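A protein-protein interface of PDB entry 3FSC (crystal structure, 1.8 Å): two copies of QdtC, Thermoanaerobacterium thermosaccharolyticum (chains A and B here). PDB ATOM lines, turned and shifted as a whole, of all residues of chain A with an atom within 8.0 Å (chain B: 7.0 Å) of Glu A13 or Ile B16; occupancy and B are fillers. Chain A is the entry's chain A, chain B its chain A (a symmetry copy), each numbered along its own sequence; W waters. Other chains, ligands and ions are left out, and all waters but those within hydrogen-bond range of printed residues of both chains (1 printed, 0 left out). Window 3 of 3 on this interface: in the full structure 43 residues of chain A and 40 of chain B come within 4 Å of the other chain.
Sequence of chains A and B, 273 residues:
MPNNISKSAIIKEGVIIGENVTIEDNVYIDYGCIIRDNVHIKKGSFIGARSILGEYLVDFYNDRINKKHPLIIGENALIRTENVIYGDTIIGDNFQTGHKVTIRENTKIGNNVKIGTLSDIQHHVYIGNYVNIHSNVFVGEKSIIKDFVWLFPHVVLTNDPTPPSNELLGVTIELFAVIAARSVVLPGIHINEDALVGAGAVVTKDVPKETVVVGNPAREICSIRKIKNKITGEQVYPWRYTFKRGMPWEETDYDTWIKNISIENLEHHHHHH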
ATOM      1  N   ILE A  10     -35.259  -4.433 -15.676  1.00  0.00           N
ATOM      2  CA  ILE A  10     -33.842  -4.474 -15.276  1.00  0.00           C
ATOM      3  C   ILE A  10     -33.496  -2.993 -15.120  1.00  0.00           C
ATOM      4  O   ILE A  10     -33.645  -2.229 -16.070  1.00  0.00           O
ATOM      5  CB  ILE A  10     -32.920  -4.975 -16.407  1.00  0.00           C
ATOM      6  CG1 ILE A  10     -33.126  -6.465 -16.683  1.00  0.00           C
ATOM      7  CG2 ILE A  10     -31.489  -4.692 -16.044  1.00  0.00           C
ATOM      8  CD1 ILE A  10     -32.989  -7.325 -15.442  1.00  0.00           C
ATOM      9  N   ILE A  11     -33.054  -2.587 -13.940  1.00  0.00           N
ATOM     10  CA  ILE A  11     -32.742  -1.200 -13.644  1.00  0.00           C
ATOM     11  C   ILE A  11     -31.285  -1.163 -13.226  1.00  0.00           C
ATOM     12  O   ILE A  11     -30.938  -1.544 -12.104  1.00  0.00           O
ATOM     13  CB  ILE A  11     -33.564  -0.685 -12.426  1.00  0.00           C
ATOM     14  CG1 ILE A  11     -35.061  -0.932 -12.533  1.00  0.00           C
ATOM     15  CG2 ILE A  11     -33.212   0.755 -11.994  1.00  0.00           C
ATOM     16  CD1 ILE A  11     -35.736  -0.215 -13.624  1.00  0.00           C
ATOM     17  N   LYS A  12     -30.425  -0.693 -14.118  1.00  0.00           N
ATOM     18  CA  LYS A  12     -29.005  -0.651 -13.811  1.00  0.00           C
ATOM     19  C   LYS A  12     -28.575   0.314 -12.724  1.00  0.00           C
ATOM     20  O   LYS A  12     -29.329   1.143 -12.230  1.00  0.00           O
ATOM     21  CB  LYS A  12     -28.146  -0.486 -15.095  1.00  0.00           C
ATOM     22  CG  LYS A  12     -28.618  -1.364 -16.252  1.00  0.00           C
ATOM     23  CD  LYS A  12     -28.261  -2.859 -16.093  1.00  0.00           C
ATOM     24  CE  LYS A  12     -26.886  -3.146 -15.543  1.00  0.00           C
ATOM     25  NZ  LYS A  12     -26.614  -4.581 -15.815  1.00  0.00           N
ATOM     26  N   GLU A  13     -27.313   0.260 -12.329  1.00  0.00           N
ATOM     27  CA  GLU A  13     -27.042   1.243 -11.300  1.00  0.00           C
ATOM     28  C   GLU A  13     -26.914   2.678 -11.773  1.00  0.00           C
ATOM     29  O   GLU A  13     -26.727   2.987 -12.952  1.00  0.00           O
ATOM     30  CB  GLU A  13     -25.850   0.831 -10.476  1.00  0.00           C
ATOM     31  CG  GLU A  13     -24.762   0.507 -11.424  1.00  0.00           C
ATOM     32  CD  GLU A  13     -23.417   0.666 -10.771  1.00  0.00           C
ATOM     33  OE1 GLU A  13     -22.485  -0.104 -11.100  1.00  0.00           O
ATOM     34  OE2 GLU A  13     -23.324   1.575  -9.918  1.00  0.00           O
ATOM     35  N   GLY A  14     -27.016   3.550 -10.783  1.00  0.00           N
ATOM     36  CA  GLY A  14     -26.922   4.984 -10.999  1.00  0.00           C
ATOM     37  C   GLY A  14     -28.309   5.459 -11.376  1.00  0.00           C
ATOM     38  O   GLY A  14     -28.566   6.668 -11.375  1.00  0.00           O
ATOM     39  N   VAL A  15     -29.208   4.533 -11.708  1.00  0.00           N
ATOM     40  CA  VAL A  15     -30.528   5.035 -12.053  1.00  0.00           C
ATOM     41  C   VAL A  15     -31.208   5.797 -10.902  1.00  0.00           C
ATOM     42  O   VAL A  15     -31.106   5.399  -9.753  1.00  0.00           O
ATOM     43  CB  VAL A  15     -31.376   3.931 -12.672  1.00  0.00           C
ATOM     44  CG1 VAL A  15     -32.777   4.438 -12.960  1.00  0.00           C
ATOM     45  CG2 VAL A  15     -30.684   3.424 -13.934  1.00  0.00           C
ATOM     46  N   ILE A  16     -31.856   6.922 -11.197  1.00  0.00           N
ATOM     47  CA  ILE A  16     -32.542   7.744 -10.197  1.00  0.00           C
ATOM     48  C   ILE A  16     -34.001   7.754 -10.622  1.00  0.00           C
ATOM     49  O   ILE A  16     -34.312   8.112 -11.755  1.00  0.00           O
ATOM     50  CB  ILE A  16     -32.044   9.237 -10.055  1.00  0.00           C
ATOM     51  CG1 ILE A  16     -30.614   9.338  -9.512  1.00  0.00           C
ATOM     52  CG2 ILE A  16     -32.978   9.973  -9.093  1.00  0.00           C
ATOM     53  CD1 ILE A  16     -30.211   8.088  -8.766  1.00  0.00           C
ATOM     54  N   ILE A  29     -33.567  -0.270 -18.088  1.00  0.00           N
ATOM     55  CA  ILE A  29     -33.095   1.097 -17.907  1.00  0.00           C
ATOM     56  C   ILE A  29     -31.636   1.050 -17.588  1.00  0.00           C
ATOM     57  O   ILE A  29     -31.234   0.650 -16.487  1.00  0.00           O
ATOM     58  CB  ILE A  29     -33.814   1.779 -16.765  1.00  0.00           C
ATOM     59  CG1 ILE A  29     -35.294   1.449 -16.944  1.00  0.00           C
ATOM     60  CG2 ILE A  29     -33.513   3.261 -16.830  1.00  0.00           C
ATOM     61  CD1 ILE A  29     -36.177   2.561 -16.618  1.00  0.00           C
ATOM     62  N   ASP A  30     -30.867   1.464 -18.584  1.00  0.00           N
ATOM     63  CA  ASP A  30     -29.415   1.478 -18.518  1.00  0.00           C
ATOM     64  C   ASP A  30     -28.773   2.432 -17.520  1.00  0.00           C
ATOM     65  O   ASP A  30     -29.419   3.360 -16.980  1.00  0.00           O
ATOM     66  CB  ASP A  30     -28.810   1.560 -19.939  1.00  0.00           C
ATOM     67  CG  ASP A  30     -27.522   0.745 -20.097  1.00  0.00           C
ATOM     68  OD1 ASP A  30     -27.023   0.176 -19.114  1.00  0.00           O
ATOM     69  OD2 ASP A  30     -26.966   0.655 -21.208  1.00  0.00           O
ATOM     70  N   TYR A  31     -27.477   2.211 -17.286  1.00  0.00           N
ATOM     71  CA  TYR A  31     -26.797   3.084 -16.329  1.00  0.00           C
ATOM     72  C   TYR A  31     -27.103   4.568 -16.271  1.00  0.00           C
ATOM     73  O   TYR A  31     -27.074   5.292 -17.270  1.00  0.00           O
ATOM     74  CB  TYR A  31     -25.286   3.017 -16.493  1.00  0.00           C
ATOM     75  CG  TYR A  31     -24.721   1.638 -16.378  1.00  0.00           C
ATOM     76  CD1 TYR A  31     -24.699   0.974 -15.140  1.00  0.00           C
ATOM     77  CD2 TYR A  31     -24.173   1.012 -17.500  1.00  0.00           C
ATOM     78  CE1 TYR A  31     -24.156  -0.310 -15.040  1.00  0.00           C
ATOM     79  CE2 TYR A  31     -23.637  -0.271 -17.416  1.00  0.00           C
ATOM     80  CZ  TYR A  31     -23.660  -0.905 -16.180  1.00  0.00           C
ATOM     81  OH  TYR A  31     -23.137  -2.154 -16.056  1.00  0.00           O
ATOM     82  N   GLY A  32     -27.339   5.015 -15.051  1.00  0.00           N
ATOM     83  CA  GLY A  32     -27.521   6.420 -14.801  1.00  0.00           C
ATOM     84  C   GLY A  32     -28.688   7.187 -15.329  1.00  0.00           C
ATOM     85  O   GLY A  32     -28.679   8.415 -15.250  1.00  0.00           O
ATOM     86  N   CYS A  33     -29.721   6.515 -15.805  1.00  0.00           N
ATOM     87  CA  CYS A  33     -30.798   7.375 -16.258  1.00  0.00           C
ATOM     88  C   CYS A  33     -31.474   8.065 -15.098  1.00  0.00           C
ATOM     89  O   CYS A  33     -31.519   7.578 -13.972  1.00  0.00           O
ATOM     90  CB  CYS A  33     -31.883   6.524 -16.858  1.00  0.00           C
ATOM     91  SG  CYS A  33     -31.390   5.734 -18.396  1.00  0.00           S
ATOM     92  N   ALA A  49     -28.488   4.675 -21.476  1.00  0.00           N
ATOM     93  CA  ALA A  49     -27.649   5.227 -20.431  1.00  0.00           C
ATOM     94  C   ALA A  49     -27.767   6.721 -20.283  1.00  0.00           C
ATOM     95  O   ALA A  49     -27.625   7.444 -21.250  1.00  0.00           O
ATOM     96  CB  ALA A  49     -26.194   4.814 -20.643  1.00  0.00           C
ATOM     97  N   ARG A  50     -27.969   7.179 -19.057  1.00  0.00           N
ATOM     98  CA  ARG A  50     -27.999   8.613 -18.834  1.00  0.00           C
ATOM     99  C   ARG A  50     -29.048   9.469 -19.465  1.00  0.00           C
ATOM    100  O   ARG A  50     -28.942  10.681 -19.450  1.00  0.00           O
ATOM    101  CB  ARG A  50     -26.627   9.264 -18.960  1.00  0.00           C
ATOM    102  CG  ARG A  50     -25.665   8.520 -18.028  1.00  0.00           C
ATOM    103  CD  ARG A  50     -24.456   9.328 -17.629  1.00  0.00           C
ATOM    104  NE  ARG A  50     -23.270   8.870 -18.354  1.00  0.00           N
ATOM    105  CZ  ARG A  50     -22.431   7.907 -17.976  1.00  0.00           C
ATOM    106  NH1 ARG A  50     -22.584   7.204 -16.836  1.00  0.00           N
ATOM    107  NH2 ARG A  50     -21.419   7.677 -18.802  1.00  0.00           N
ATOM    108  N   ILE B  11      -8.358   5.857 -12.828  1.00  0.00           N
ATOM    109  CA  ILE B  11      -9.749   5.575 -13.137  1.00  0.00           C
ATOM    110  C   ILE B  11     -10.580   6.310 -12.102  1.00  0.00           C
ATOM    111  O   ILE B  11     -10.685   5.876 -10.951  1.00  0.00           O
ATOM    112  CB  ILE B  11     -10.069   4.061 -12.967  1.00  0.00           C
ATOM    113  CG1 ILE B  11      -9.114   3.134 -13.703  1.00  0.00           C
ATOM    114  CG2 ILE B  11     -11.557   3.705 -13.186  1.00  0.00           C
ATOM    115  CD1 ILE B  11      -9.141   3.243 -15.168  1.00  0.00           C
ATOM    116  N   LYS B  12     -11.185   7.416 -12.507  1.00  0.00           N
ATOM    117  CA  LYS B  12     -11.977   8.199 -11.571  1.00  0.00           C
ATOM    118  C   LYS B  12     -13.251   7.556 -11.059  1.00  0.00           C
ATOM    119  O   LYS B  12     -13.702   6.513 -11.513  1.00  0.00           O
ATOM    120  CB  LYS B  12     -12.233   9.636 -12.100  1.00  0.00           C
ATOM    121  CG  LYS B  12     -10.997  10.278 -12.726  1.00  0.00           C
ATOM    122  CD  LYS B  12      -9.943  10.745 -11.697  1.00  0.00           C
ATOM    123  CE  LYS B  12     -10.490  11.401 -10.454  1.00  0.00           C
ATOM    124  NZ  LYS B  12      -9.346  12.087  -9.799  1.00  0.00           N
ATOM    125  N   GLU B  13     -13.905   8.188 -10.099  1.00  0.00           N
ATOM    126  CA  GLU B  13     -15.105   7.469  -9.719  1.00  0.00           C
ATOM    127  C   GLU B  13     -16.270   7.569 -10.684  1.00  0.00           C
ATOM    128  O   GLU B  13     -16.348   8.433 -11.561  1.00  0.00           O
ATOM    129  CB  GLU B  13     -15.523   7.839  -8.319  1.00  0.00           C
ATOM    130  CG  GLU B  13     -15.554   9.317  -8.254  1.00  0.00           C
ATOM    131  CD  GLU B  13     -16.488   9.786  -7.174  1.00  0.00           C
ATOM    132  OE1 GLU B  13     -16.211  10.831  -6.540  1.00  0.00           O
ATOM    133  OE2 GLU B  13     -17.498   9.077  -6.975  1.00  0.00           O
ATOM    134  N   GLY B  14     -17.186   6.639 -10.472  1.00  0.00           N
ATOM    135  CA  GLY B  14     -18.393   6.541 -11.276  1.00  0.00           C
ATOM    136  C   GLY B  14     -18.037   5.718 -12.496  1.00  0.00           C
ATOM    137  O   GLY B  14     -18.935   5.275 -13.221  1.00  0.00           O
ATOM    138  N   VAL B  15     -16.745   5.511 -12.745  1.00  0.00           N
ATOM    139  CA  VAL B  15     -16.452   4.707 -13.920  1.00  0.00           C
ATOM    140  C   VAL B  15     -17.035   3.285 -13.844  1.00  0.00           C
ATOM    141  O   VAL B  15     -17.013   2.665 -12.792  1.00  0.00           O
ATOM    142  CB  VAL B  15     -14.968   4.769 -14.255  1.00  0.00           C
ATOM    143  CG1 VAL B  15     -14.654   3.869 -15.436  1.00  0.00           C
ATOM    144  CG2 VAL B  15     -14.582   6.219 -14.528  1.00  0.00           C
ATOM    145  N   ILE B  16     -17.605   2.785 -14.939  1.00  0.00           N
ATOM    146  CA  ILE B  16     -18.200   1.448 -15.000  1.00  0.00           C
ATOM    147  C   ILE B  16     -17.406   0.708 -16.064  1.00  0.00           C
ATOM    148  O   ILE B  16     -17.296   1.179 -17.193  1.00  0.00           O
ATOM    149  CB  ILE B  16     -19.734   1.379 -15.371  1.00  0.00           C
ATOM    150  CG1 ILE B  16     -20.635   1.996 -14.295  1.00  0.00           C
ATOM    151  CG2 ILE B  16     -20.128  -0.088 -15.547  1.00  0.00           C
ATOM    152  CD1 ILE B  16     -19.944   2.045 -12.952  1.00  0.00           C
ATOM    153  N   ILE B  17     -16.836  -0.442 -15.712  1.00  0.00           N
ATOM    154  CA  ILE B  17     -16.045  -1.247 -16.642  1.00  0.00           C
ATOM    155  C   ILE B  17     -16.614  -2.627 -16.929  1.00  0.00           C
ATOM    156  O   ILE B  17     -17.038  -3.317 -15.999  1.00  0.00           O
ATOM    157  CB  ILE B  17     -14.633  -1.349 -16.109  1.00  0.00           C
ATOM    158  CG1 ILE B  17     -14.247   0.060 -15.649  1.00  0.00           C
ATOM    159  CG2 ILE B  17     -13.780  -2.156 -17.078  1.00  0.00           C
ATOM    160  CD1 ILE B  17     -12.760   0.324 -15.557  1.00  0.00           C
ATOM    161  N   GLY B  18     -16.634  -3.033 -18.201  1.00  0.00           N
ATOM    162  CA  GLY B  18     -17.212  -4.333 -18.532  1.00  0.00           C
ATOM    163  C   GLY B  18     -16.171  -5.440 -18.539  1.00  0.00           C
ATOM    164  O   GLY B  18     -15.210  -5.412 -17.761  1.00  0.00           O
ATOM    165  N   ILE B  29      -9.109   7.803 -17.127  1.00  0.00           N
ATOM    166  CA  ILE B  29     -10.534   7.718 -17.423  1.00  0.00           C
ATOM    167  C   ILE B  29     -11.272   8.538 -16.415  1.00  0.00           C
ATOM    168  O   ILE B  29     -11.382   8.160 -15.241  1.00  0.00           O
ATOM    169  CB  ILE B  29     -11.027   6.290 -17.335  1.00  0.00           C
ATOM    170  CG1 ILE B  29      -9.993   5.442 -18.071  1.00  0.00           C
ATOM    171  CG2 ILE B  29     -12.409   6.227 -17.948  1.00  0.00           C
ATOM    172  CD1 ILE B  29     -10.581   4.360 -18.848  1.00  0.00           C
ATOM    173  N   GLY B  32     -17.281   8.986 -14.340  1.00  0.00           N
ATOM    174  CA  GLY B  32     -18.437   8.384 -14.947  1.00  0.00           C
ATOM    175  C   GLY B  32     -18.401   7.754 -16.301  1.00  0.00           C
ATOM    176  O   GLY B  32     -19.461   7.442 -16.842  1.00  0.00           O
ATOM    177  N   CYS B  33     -17.225   7.496 -16.844  1.00  0.00           N
ATOM    178  CA  CYS B  33     -17.328   6.858 -18.143  1.00  0.00           C
ATOM    179  C   CYS B  33     -17.853   5.449 -18.023  1.00  0.00           C
ATOM    180  O   CYS B  33     -17.680   4.760 -17.022  1.00  0.00           O
ATOM    181  CB  CYS B  33     -15.947   6.685 -18.713  1.00  0.00           C
ATOM    182  SG  CYS B  33     -15.161   8.245 -19.143  1.00  0.00           S
ATOM    183  N   ILE B  34     -18.451   4.993 -19.108  1.00  0.00           N
ATOM    184  CA  ILE B  34     -18.919   3.631 -19.144  1.00  0.00           C
ATOM    185  C   ILE B  34     -18.065   2.977 -20.215  1.00  0.00           C
ATOM    186  O   ILE B  34     -18.015   3.400 -21.386  1.00  0.00           O
ATOM    187  CB  ILE B  34     -20.387   3.527 -19.494  1.00  0.00           C
ATOM    188  CG1 ILE B  34     -21.210   4.097 -18.344  1.00  0.00           C
ATOM    189  CG2 ILE B  34     -20.743   2.102 -19.777  1.00  0.00           C
ATOM    190  CD1 ILE B  34     -22.593   4.403 -18.886  1.00  0.00           C
ATOM    191  N   ILE B  35     -17.347   1.960 -19.756  1.00  0.00           N
ATOM    192  CA  ILE B  35     -16.486   1.197 -20.645  1.00  0.00           C
ATOM    193  C   ILE B  35     -17.201  -0.131 -20.766  1.00  0.00           C
ATOM    194  O   ILE B  35     -17.190  -0.925 -19.828  1.00  0.00           O
ATOM    195  CB  ILE B  35     -15.061   0.980 -20.124  1.00  0.00           C
ATOM    196  CG1 ILE B  35     -14.461   2.285 -19.612  1.00  0.00           C
ATOM    197  CG2 ILE B  35     -14.190   0.580 -21.302  1.00  0.00           C
ATOM    198  CD1 ILE B  35     -14.204   3.286 -20.735  1.00  0.00           C
ATOM    199  N   ARG B  36     -17.836  -0.347 -21.910  1.00  0.00           N
ATOM    200  CA  ARG B  36     -18.555  -1.584 -22.150  1.00  0.00           C
ATOM    201  C   ARG B  36     -17.515  -2.640 -22.567  1.00  0.00           C
ATOM    202  O   ARG B  36     -16.322  -2.355 -22.726  1.00  0.00           O
ATOM    203  CB  ARG B  36     -19.679  -1.404 -23.206  1.00  0.00           C
ATOM    204  CG  ARG B  36     -20.535  -0.177 -22.954  1.00  0.00           C
ATOM    205  CD  ARG B  36     -21.852  -0.386 -23.669  1.00  0.00           C
ATOM    206  NE  ARG B  36     -22.846   0.686 -23.684  1.00  0.00           N
ATOM    207  CZ  ARG B  36     -23.770   0.961 -22.765  1.00  0.00           C
ATOM    208  NH1 ARG B  36     -24.607   1.960 -23.031  1.00  0.00           N
ATOM    209  NH2 ARG B  36     -23.878   0.315 -21.596  1.00  0.00           N
HETATM  210  O   HOH W   1     -27.379   2.361 -22.870  1.00  0.00           O
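O of Gly B32 lies within hydrogen-bond range of NH2 of Arg A50, 2.8 Å away.
The guanidinium group (NH2) of Arg B36 is in salt-bridge range of the side-chain carboxylate (OD2) of Asp A30, at 3.1 Å.
The backbone carbonyl oxygen (O) of Glu A13 sits at hydrogen-bond distance from the backbone NH (N) of Gly A32.
The backbone carbonyl oxygen (O) of Tyr A31 sits at hydrogen-bond distance from the backbone NH (N) of Arg A50.
The backbone NH (N) of Ile B16 is in hydrogen-bond range of the backbone carbonyl oxygen (O) of Cys B33.
SG of Cys A33 sits at hydrogen-bond distance from N of Arg A50 (3.8 Å).
The side-chain sulfur (SG) of Cys A33 sits at hydrogen-bond distance from the backbone carbonyl oxygen (O) of Asp A30 (3.4 Å).
The backbone NH (N) of Gly B32 is in hydrogen-bond range of the backbone carbonyl oxygen (O) of Glu B13.
Among the printed residues, merely in contact across the chains: Glu A13 with Ile B16, Tyr A31 with Ile B16, Tyr A31 with Ile B34 and Arg A50 with Ile B34.
Glu A13 touches just one residue of chain B: Ile B16.
Of chain A, only Glu A13 and Tyr A31 come within 4 Å of Ile B16.
Of the printed residues of chain A, Arg B36 touches Asp A30 (3.1 Å).
Printed residues of chain B within 4 Å of Tyr A31: Ile B16 (3.7 Å) and Ile B34 (3.9 Å).
Printed residues of chain A within 4 Å of Gly B32: Arg A50 (2.8 Å).
Of the printed residues of chain B, Asp A30 touches Arg B36 (3.1 Å).
Ile B29 touches none of the printed residues of chain A.
The nearest residue of chain B that does not touch Glu A13 is Val B15 (6.4 Å).
The nearest printed residue of chain A that does not touch Arg B36 is Ala A49 (4.05 Å).
Of the 14 printed residues of chain A, 4 touch a printed residue of chain B.
Hydrophobic or aromatic side chains of chain A that line the printed part of chain B: Tyr A31.
Of the 14 printed residues of chain B, 4 touch a printed residue of chain A.
Printed residues of chain B that touch a printed residue of chain A: Ile B16, Gly B32, Ile B34 and Arg B36.
Hydrophobic or aromatic side chains of chain B within 4 Å of the printed part of chain A: Ile B16 and Ile B34.
Along chain B the printed residues that touch a printed residue of chain A span positions 16 to 36.
Among the printed residues, Asp or Glu carboxylates within 4 Å of a Lys or Arg side-chain nitrogen of the other chain: Asp A30 with Arg B36 (3.1 Å).
Glu A13 touches Ile B16, but with the chains exchanged Ile A16 does not touch Glu B13 (12.9 Å).
Positions printed for both chains: 11, 12, 13, 14, 15, 16, 29, 32 and 33.
Water W1 lies within hydrogen-bond range of OD2 of Asp A30 (2.4 Å), NH1 of Arg B36 (2.8 Å) and N of Ala A49 (2.9 Å).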
